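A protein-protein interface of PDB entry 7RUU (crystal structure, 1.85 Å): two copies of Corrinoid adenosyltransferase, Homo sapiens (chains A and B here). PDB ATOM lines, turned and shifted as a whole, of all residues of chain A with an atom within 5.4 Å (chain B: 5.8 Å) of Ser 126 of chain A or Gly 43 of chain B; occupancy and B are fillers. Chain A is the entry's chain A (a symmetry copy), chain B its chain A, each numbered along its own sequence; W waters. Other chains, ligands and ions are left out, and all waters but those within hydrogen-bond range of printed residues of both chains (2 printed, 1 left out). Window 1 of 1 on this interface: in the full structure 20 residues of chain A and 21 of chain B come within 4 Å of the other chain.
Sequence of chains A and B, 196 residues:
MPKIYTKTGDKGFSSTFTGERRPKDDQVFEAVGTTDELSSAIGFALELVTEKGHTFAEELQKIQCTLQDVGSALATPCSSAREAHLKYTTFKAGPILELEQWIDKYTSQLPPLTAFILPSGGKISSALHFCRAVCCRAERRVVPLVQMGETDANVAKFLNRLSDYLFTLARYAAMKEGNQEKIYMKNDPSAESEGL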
ATOM      1  N   PRO A 119     -17.444   3.001  16.571  1.00  0.00           N
ATOM      2  CA  PRO A 119     -17.319   4.336  17.178  1.00  0.00           C
ATOM      3  C   PRO A 119     -18.562   5.155  16.883  1.00  0.00           C
ATOM      4  O   PRO A 119     -18.775   5.600  15.753  1.00  0.00           O
ATOM      5  CB  PRO A 119     -16.072   4.939  16.511  1.00  0.00           C
ATOM      6  CG  PRO A 119     -15.443   3.881  15.729  1.00  0.00           C
ATOM      7  CD  PRO A 119     -16.432   2.753  15.531  1.00  0.00           C
ATOM      8  N   SER A 120     -19.412   5.316  17.886  1.00  0.00           N
ATOM      9  CA  SER A 120     -20.636   6.082  17.754  1.00  0.00           C
ATOM     10  C   SER A 120     -21.124   6.412  19.152  1.00  0.00           C
ATOM     11  O   SER A 120     -20.332   6.867  19.985  1.00  0.00           O
ATOM     12  CB  SER A 120     -21.682   5.304  16.953  1.00  0.00           C
ATOM     13  OG  SER A 120     -21.924   4.061  17.570  1.00  0.00           O
ATOM     14  N   GLY A 121     -22.405   6.188  19.428  1.00  0.00           N
ATOM     15  CA  GLY A 121     -22.932   6.359  20.773  1.00  0.00           C
ATOM     16  C   GLY A 121     -23.470   7.731  21.115  1.00  0.00           C
ATOM     17  O   GLY A 121     -23.686   8.017  22.297  1.00  0.00           O
ATOM     18  N   GLY A 122     -23.715   8.589  20.137  1.00  0.00           N
ATOM     19  CA  GLY A 122     -24.096   9.958  20.416  1.00  0.00           C
ATOM     20  C   GLY A 122     -23.011  10.937  19.997  1.00  0.00           C
ATOM     21  O   GLY A 122     -21.891  10.566  19.645  1.00  0.00           O
ATOM     22  N   LYS A 123     -23.377  12.221  20.021  1.00  0.00           N
ATOM     23  CA  LYS A 123     -22.480  13.254  19.508  1.00  0.00           C
ATOM     24  C   LYS A 123     -21.212  13.348  20.345  1.00  0.00           C
ATOM     25  O   LYS A 123     -20.095  13.331  19.813  1.00  0.00           O
ATOM     26  CB  LYS A 123     -23.195  14.606  19.481  1.00  0.00           C
ATOM     27  CG  LYS A 123     -23.303  15.241  18.118  1.00  0.00           C
ATOM     28  CD  LYS A 123     -23.569  16.725  18.286  1.00  0.00           C
ATOM     29  CE  LYS A 123     -24.238  17.323  17.089  1.00  0.00           C
ATOM     30  NZ  LYS A 123     -24.383  18.779  17.306  1.00  0.00           N
ATOM     31  N   ILE A 124     -21.371  13.434  21.667  1.00  0.00           N
ATOM     32  CA  ILE A 124     -20.227  13.535  22.567  1.00  0.00           C
ATOM     33  C   ILE A 124     -19.357  12.287  22.466  1.00  0.00           C
ATOM     34  O   ILE A 124     -18.127  12.371  22.343  1.00  0.00           O
ATOM     35  CB  ILE A 124     -20.715  13.765  24.009  1.00  0.00           C
ATOM     36  CG1 ILE A 124     -21.278  15.180  24.139  1.00  0.00           C
ATOM     37  CG2 ILE A 124     -19.602  13.500  25.003  1.00  0.00           C
ATOM     38  CD1 ILE A 124     -22.023  15.431  25.430  1.00  0.00           C
ATOM     39  N   SER A 125     -19.985  11.109  22.536  1.00  0.00           N
ATOM     40  CA  SER A 125     -19.238   9.858  22.473  1.00  0.00           C
ATOM     41  C   SER A 125     -18.478   9.727  21.153  1.00  0.00           C
ATOM     42  O   SER A 125     -17.299   9.358  21.149  1.00  0.00           O
ATOM     43  CB  SER A 125     -20.193   8.680  22.699  1.00  0.00           C
ATOM     44  OG  SER A 125     -19.631   7.445  22.284  1.00  0.00           O
ATOM     45  N   SER A 126     -19.122  10.059  20.024  1.00  0.00           N
ATOM     46  CA  SER A 126     -18.427   9.931  18.747  1.00  0.00           C
ATOM     47  C   SER A 126     -17.291  10.947  18.627  1.00  0.00           C
ATOM     48  O   SER A 126     -16.247  10.641  18.037  1.00  0.00           O
ATOM     49  CB  SER A 126     -19.409  10.063  17.571  1.00  0.00           C
ATOM     50  OG  SER A 126     -19.892  11.387  17.441  1.00  0.00           O
ATOM     51  N   ALA A 127     -17.474  12.159  19.171  1.00  0.00           N
ATOM     52  CA  ALA A 127     -16.388  13.136  19.167  1.00  0.00           C
ATOM     53  C   ALA A 127     -15.232  12.656  20.039  1.00  0.00           C
ATOM     54  O   ALA A 127     -14.060  12.842  19.694  1.00  0.00           O
ATOM     55  CB  ALA A 127     -16.880  14.504  19.664  1.00  0.00           C
ATOM     56  N   LEU A 128     -15.546  12.018  21.173  1.00  0.00           N
ATOM     57  CA  LEU A 128     -14.483  11.477  22.009  1.00  0.00           C
ATOM     58  C   LEU A 128     -13.754  10.320  21.334  1.00  0.00           C
ATOM     59  O   LEU A 128     -12.544  10.163  21.531  1.00  0.00           O
ATOM     60  CB  LEU A 128     -15.048  11.052  23.375  1.00  0.00           C
ATOM     61  CG  LEU A 128     -15.452  12.226  24.286  1.00  0.00           C
ATOM     62  CD1 LEU A 128     -16.230  11.670  25.488  1.00  0.00           C
ATOM     63  CD2 LEU A 128     -14.241  13.073  24.767  1.00  0.00           C
ATOM     64  N   HIS A 129     -14.448   9.496  20.541  1.00  0.00           N
ATOM     65  CA  HIS A 129     -13.730   8.446  19.814  1.00  0.00           C
ATOM     66  C   HIS A 129     -12.803   9.035  18.760  1.00  0.00           C
ATOM     67  O   HIS A 129     -11.742   8.460  18.477  1.00  0.00           O
ATOM     68  CB  HIS A 129     -14.704   7.463  19.151  1.00  0.00           C
ATOM     69  CG  HIS A 129     -15.267   6.441  20.096  1.00  0.00           C
ATOM     70  ND1 HIS A 129     -14.473   5.592  20.837  1.00  0.00           N
ATOM     71  CD2 HIS A 129     -16.548   6.141  20.422  1.00  0.00           C
ATOM     72  CE1 HIS A 129     -15.244   4.819  21.590  1.00  0.00           C
ATOM     73  NE2 HIS A 129     -16.506   5.128  21.354  1.00  0.00           N
ATOM     74  N   PHE A 130     -13.188  10.159  18.150  1.00  0.00           N
ATOM     75  CA  PHE A 130     -12.258  10.818  17.241  1.00  0.00           C
ATOM     76  C   PHE A 130     -11.038  11.334  18.003  1.00  0.00           C
ATOM     77  O   PHE A 130      -9.888  11.105  17.599  1.00  0.00           O
ATOM     78  CB  PHE A 130     -12.966  11.950  16.482  1.00  0.00           C
ATOM     79  CG  PHE A 130     -12.066  12.666  15.520  1.00  0.00           C
ATOM     80  CD1 PHE A 130     -11.667  12.040  14.341  1.00  0.00           C
ATOM     81  CD2 PHE A 130     -11.568  13.927  15.820  1.00  0.00           C
ATOM     82  CE1 PHE A 130     -10.796  12.686  13.459  1.00  0.00           C
ATOM     83  CE2 PHE A 130     -10.709  14.576  14.948  1.00  0.00           C
ATOM     84  CZ  PHE A 130     -10.328  13.958  13.764  1.00  0.00           C
ATOM     85  N   CYS A 131     -11.274  11.989  19.142  1.00  0.00           N
ATOM     86  CA  CYS A 131     -10.188  12.414  20.018  1.00  0.00           C
ATOM     87  C   CYS A 131      -9.279  11.233  20.372  1.00  0.00           C
ATOM     88  O   CYS A 131      -8.048  11.368  20.449  1.00  0.00           O
ATOM     89  CB  CYS A 131     -10.767  12.993  21.302  1.00  0.00           C
ATOM     90  SG  CYS A 131     -11.519  14.605  21.126  1.00  0.00           S
ATOM     91  N   LEU B  38     -10.565   7.235  10.688  1.00  0.00           N
ATOM     92  CA  LEU B  38     -11.619   7.335   9.676  1.00  0.00           C
ATOM     93  C   LEU B  38     -12.959   6.846  10.214  1.00  0.00           C
ATOM     94  O   LEU B  38     -13.986   7.522  10.067  1.00  0.00           O
ATOM     95  CB  LEU B  38     -11.235   6.525   8.433  1.00  0.00           C
ATOM     96  CG  LEU B  38     -12.335   6.412   7.363  1.00  0.00           C
ATOM     97  CD1 LEU B  38     -12.749   7.822   6.879  1.00  0.00           C
ATOM     98  CD2 LEU B  38     -11.855   5.566   6.183  1.00  0.00           C
ATOM     99  N   SER B  39     -12.985   5.648  10.806  1.00  0.00           N
ATOM    100  CA  SER B  39     -14.252   5.117  11.295  1.00  0.00           C
ATOM    101  C   SER B  39     -14.833   6.019  12.380  1.00  0.00           C
ATOM    102  O   SER B  39     -16.056   6.191  12.468  1.00  0.00           O
ATOM    103  CB  SER B  39     -14.067   3.694  11.832  1.00  0.00           C
ATOM    104  OG  SER B  39     -15.335   3.149  12.187  1.00  0.00           O
ATOM    105  N   SER B  40     -13.975   6.604  13.208  1.00  0.00           N
ATOM    106  CA  SER B  40     -14.461   7.505  14.252  1.00  0.00           C
ATOM    107  C   SER B  40     -14.998   8.816  13.674  1.00  0.00           C
ATOM    108  O   SER B  40     -15.990   9.351  14.179  1.00  0.00           O
ATOM    109  CB  SER B  40     -13.363   7.797  15.282  1.00  0.00           C
ATOM    110  OG  SER B  40     -12.913   6.584  15.913  1.00  0.00           O
ATOM    111  N   ALA B  41     -14.329   9.381  12.664  1.00  0.00           N
ATOM    112  CA  ALA B  41     -14.876  10.569  12.010  1.00  0.00           C
ATOM    113  C   ALA B  41     -16.233  10.265  11.373  1.00  0.00           C
ATOM    114  O   ALA B  41     -17.155  11.089  11.439  1.00  0.00           O
ATOM    115  CB  ALA B  41     -13.888  11.116  10.977  1.00  0.00           C
ATOM    116  N   ILE B  42     -16.378   9.080  10.774  1.00  0.00           N
ATOM    117  CA  ILE B  42     -17.662   8.679  10.197  1.00  0.00           C
ATOM    118  C   ILE B  42     -18.722   8.543  11.288  1.00  0.00           C
ATOM    119  O   ILE B  42     -19.906   8.869  11.086  1.00  0.00           O
ATOM    120  CB  ILE B  42     -17.487   7.370   9.391  1.00  0.00           C
ATOM    121  CG1 ILE B  42     -16.712   7.660   8.103  1.00  0.00           C
ATOM    122  CG2 ILE B  42     -18.852   6.678   9.121  1.00  0.00           C
ATOM    123  CD1 ILE B  42     -16.370   6.377   7.280  1.00  0.00           C
ATOM    124  N   GLY B  43     -18.315   8.079  12.468  1.00  0.00           N
ATOM    125  CA  GLY B  43     -19.246   8.000  13.583  1.00  0.00           C
ATOM    126  C   GLY B  43     -19.822   9.351  13.963  1.00  0.00           C
ATOM    127  O   GLY B  43     -21.008   9.466  14.278  1.00  0.00           O
ATOM    128  N   PHE B  44     -18.993  10.391  13.954  1.00  0.00           N
ATOM    129  CA  PHE B  44     -19.505  11.720  14.244  1.00  0.00           C
ATOM    130  C   PHE B  44     -20.422  12.205  13.122  1.00  0.00           C
ATOM    131  O   PHE B  44     -21.500  12.745  13.391  1.00  0.00           O
ATOM    132  CB  PHE B  44     -18.349  12.690  14.472  1.00  0.00           C
ATOM    133  CG  PHE B  44     -18.791  14.080  14.841  1.00  0.00           C
ATOM    134  CD1 PHE B  44     -19.171  14.388  16.146  1.00  0.00           C
ATOM    135  CD2 PHE B  44     -18.837  15.079  13.870  1.00  0.00           C
ATOM    136  CE1 PHE B  44     -19.585  15.674  16.480  1.00  0.00           C
ATOM    137  CE2 PHE B  44     -19.255  16.362  14.200  1.00  0.00           C
ATOM    138  CZ  PHE B  44     -19.629  16.651  15.498  1.00  0.00           C
ATOM    139  N   ALA B  45     -20.031  11.995  11.860  1.00  0.00           N
ATOM    140  CA  ALA B  45     -20.915  12.369  10.752  1.00  0.00           C
ATOM    141  C   ALA B  45     -22.251  11.634  10.840  1.00  0.00           C
ATOM    142  O   ALA B  45     -23.312  12.218  10.591  1.00  0.00           O
ATOM    143  CB  ALA B  45     -20.238  12.079   9.408  1.00  0.00           C
ATOM    144  N   LEU B  46     -22.207  10.356  11.214  1.00  0.00           N
ATOM    145  CA  LEU B  46     -23.410   9.554  11.408  1.00  0.00           C
ATOM    146  C   LEU B  46     -24.341  10.171  12.452  1.00  0.00           C
ATOM    147  O   LEU B  46     -25.567  10.129  12.297  1.00  0.00           O
ATOM    148  CB  LEU B  46     -22.994   8.133  11.801  1.00  0.00           C
ATOM    149  CG  LEU B  46     -23.963   6.974  11.966  1.00  0.00           C
ATOM    150  CD1 LEU B  46     -24.874   6.942  10.783  1.00  0.00           C
ATOM    151  CD2 LEU B  46     -23.188   5.658  12.064  1.00  0.00           C
ATOM    152  N   GLU B  47     -23.784  10.764  13.513  1.00  0.00           N
ATOM    153  CA  GLU B  47     -24.631  11.425  14.505  1.00  0.00           C
ATOM    154  C   GLU B  47     -25.384  12.606  13.901  1.00  0.00           C
ATOM    155  O   GLU B  47     -26.554  12.833  14.226  1.00  0.00           O
ATOM    156  CB  GLU B  47     -23.800  11.887  15.702  1.00  0.00           C
ATOM    157  CG  GLU B  47     -23.111  10.759  16.421  1.00  0.00           C
ATOM    158  CD  GLU B  47     -24.094   9.756  17.005  1.00  0.00           C
ATOM    159  OE1 GLU B  47     -23.722   8.563  17.134  1.00  0.00           O
ATOM    160  OE2 GLU B  47     -25.240  10.166  17.326  1.00  0.00           O
ATOM    161  N   LEU B  48     -24.733  13.365  13.018  1.00  0.00           N
ATOM    162  CA  LEU B  48     -25.392  14.508  12.401  1.00  0.00           C
ATOM    163  C   LEU B  48     -26.488  14.061  11.449  1.00  0.00           C
ATOM    164  O   LEU B  48     -27.439  14.811  11.206  1.00  0.00           O
ATOM    165  CB  LEU B  48     -24.368  15.356  11.650  1.00  0.00           C
ATOM    166  CG  LEU B  48     -23.136  15.815  12.434  1.00  0.00           C
ATOM    167  CD1 LEU B  48     -22.169  16.539  11.503  1.00  0.00           C
ATOM    168  CD2 LEU B  48     -23.552  16.733  13.573  1.00  0.00           C
ATOM    169  N   GLN B  64     -18.700   1.315   8.724  1.00  0.00           N
ATOM    170  CA  GLN B  64     -17.923   1.161   9.953  1.00  0.00           C
ATOM    171  C   GLN B  64     -17.638  -0.310  10.251  1.00  0.00           C
ATOM    172  O   GLN B  64     -16.558  -0.650  10.746  1.00  0.00           O
ATOM    173  CB  GLN B  64     -18.656   1.793  11.124  1.00  0.00           C
ATOM    174  CG  GLN B  64     -18.641   3.321  11.123  1.00  0.00           C
ATOM    175  CD  GLN B  64     -19.278   3.843  12.368  1.00  0.00           C
ATOM    176  OE1 GLN B  64     -20.407   3.474  12.691  1.00  0.00           O
ATOM    177  NE2 GLN B  64     -18.549   4.663  13.110  1.00  0.00           N
HETATM  178  O   HOH W   1     -25.127   5.975  17.823  1.00  0.00           O
HETATM  179  O   HOH W   2     -22.532   3.204  14.418  1.00  0.00           O
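Pro 119 of chain A touches Ser 39 of chain B (CD to OG, 3.5 Å). O of Pro 119 of chain A touches CA of Gly 43 of chain B (3.3 Å). Glu 47 of chain B touches Ser 120 of chain A. Gly 121 of chain A touches Glu 47 of chain B (N to OE1, 3.6 Å). Lys 123 of chain A touches Phe 44 of chain B. Lys 123 of chain A touches Glu 47 of chain B (N to OE2, 3.9 Å). Ser 126 of chain A touches Gly 43 of chain B (CB to C, 3.7 Å). CA of Phe 44 of chain B touches OG of Ser 126 of chain A (3.2 Å). Ser 126 of chain A touches Glu 47 of chain B (OG to CG, 3.4 Å). Ser 40 of chain B touches Phe 130 of chain A (CB to N, 3.7 Å).
Printed residues of chain B that touch a printed residue of chain A: Ser 39, Ser 40, Gly 43, Phe 44, Glu 47, Leu 48 and Gln 64. Along chain B the printed residues that touch a printed residue of chain A span positions 39 to 64. Among the printed residues, no Asp or Glu carboxylate lies within 4 Å of a Lys or Arg side-chain nitrogen of the other chain.
No position is printed for both chains. Of the 15 pairs that touch across the chains among the printed residues, none has its exchanged pair printed and touching as well.
The backbone NH (N) of Gly 122 of chain A is in hydrogen-bond range of the side-chain carboxylate (OE1) of Glu 47 of chain B, at 3.0 Å. The side-chain hydroxyl (OG) of Ser 40 of chain B sits at hydrogen-bond distance from the backbone carbonyl oxygen (O) of His 129 of chain A, 3.4 Å away. O of Pro 119 of chain A is in hydrogen-bond range of NE2 of Gln 64 of chain B, at 2.8 Å.
The backbone NH of Gly 43 of chain B lies close to the side-chain amide nitrogen of Gln 64 of chain B, at 3.5 Å. The backbone carbonyl oxygen of Ser 120 of chain A lies within hydrogen-bond range of the backbone NH of Ser 126 of chain A (3.4 Å). O of Ser 120 of chain A sits at hydrogen-bond distance from OG of Ser 125 of chain A (2.5 Å). O of Ser 39 of chain B lies within hydrogen-bond range of NE2 of Gln 64 of chain B. O of Lys 123 of chain A lies within hydrogen-bond range of OG of Ser 126 of chain A (3.1 Å). OG of Ser 126 of chain A is in hydrogen-bond range of O of Gly 122 of chain A, at 3.1 Å.
Of the printed residues of chain B, Ser 126 of chain A touches Gly 43 (3.7 Å), Phe 44 (3.2 Å) and Glu 47 (3.4 Å). Of the printed residues of chain B, Phe 130 of chain A touches Ser 40 (3.7 Å). Printed residues of chain B within 4 Å of Pro 119 of chain A: Ser 39 (3.5 Å), Ser 40 (3.6 Å), Gly 43 (3.3 Å) and Gln 64 (2.8 Å). Ser 125 of chain A touches none of the printed residues of chain B. Ile 124 of chain A touches none of the printed residues of chain B. The nearest printed residue of chain B that does not touch Ser 126 of chain A is Ser 40 of chain B (4.1 Å). The nearest printed residue of chain A that does not touch Gly 43 of chain B is Ser 120 of chain A (4.8 Å).
Water W2 bridges OE1 of Gln 64 of chain B and OG of Ser 120 of chain A. Water W1 lies within hydrogen-bond range of OE1 of Glu 47 of chain B (3.0 Å) and N of Gly 121 of chain A (3.2 Å).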
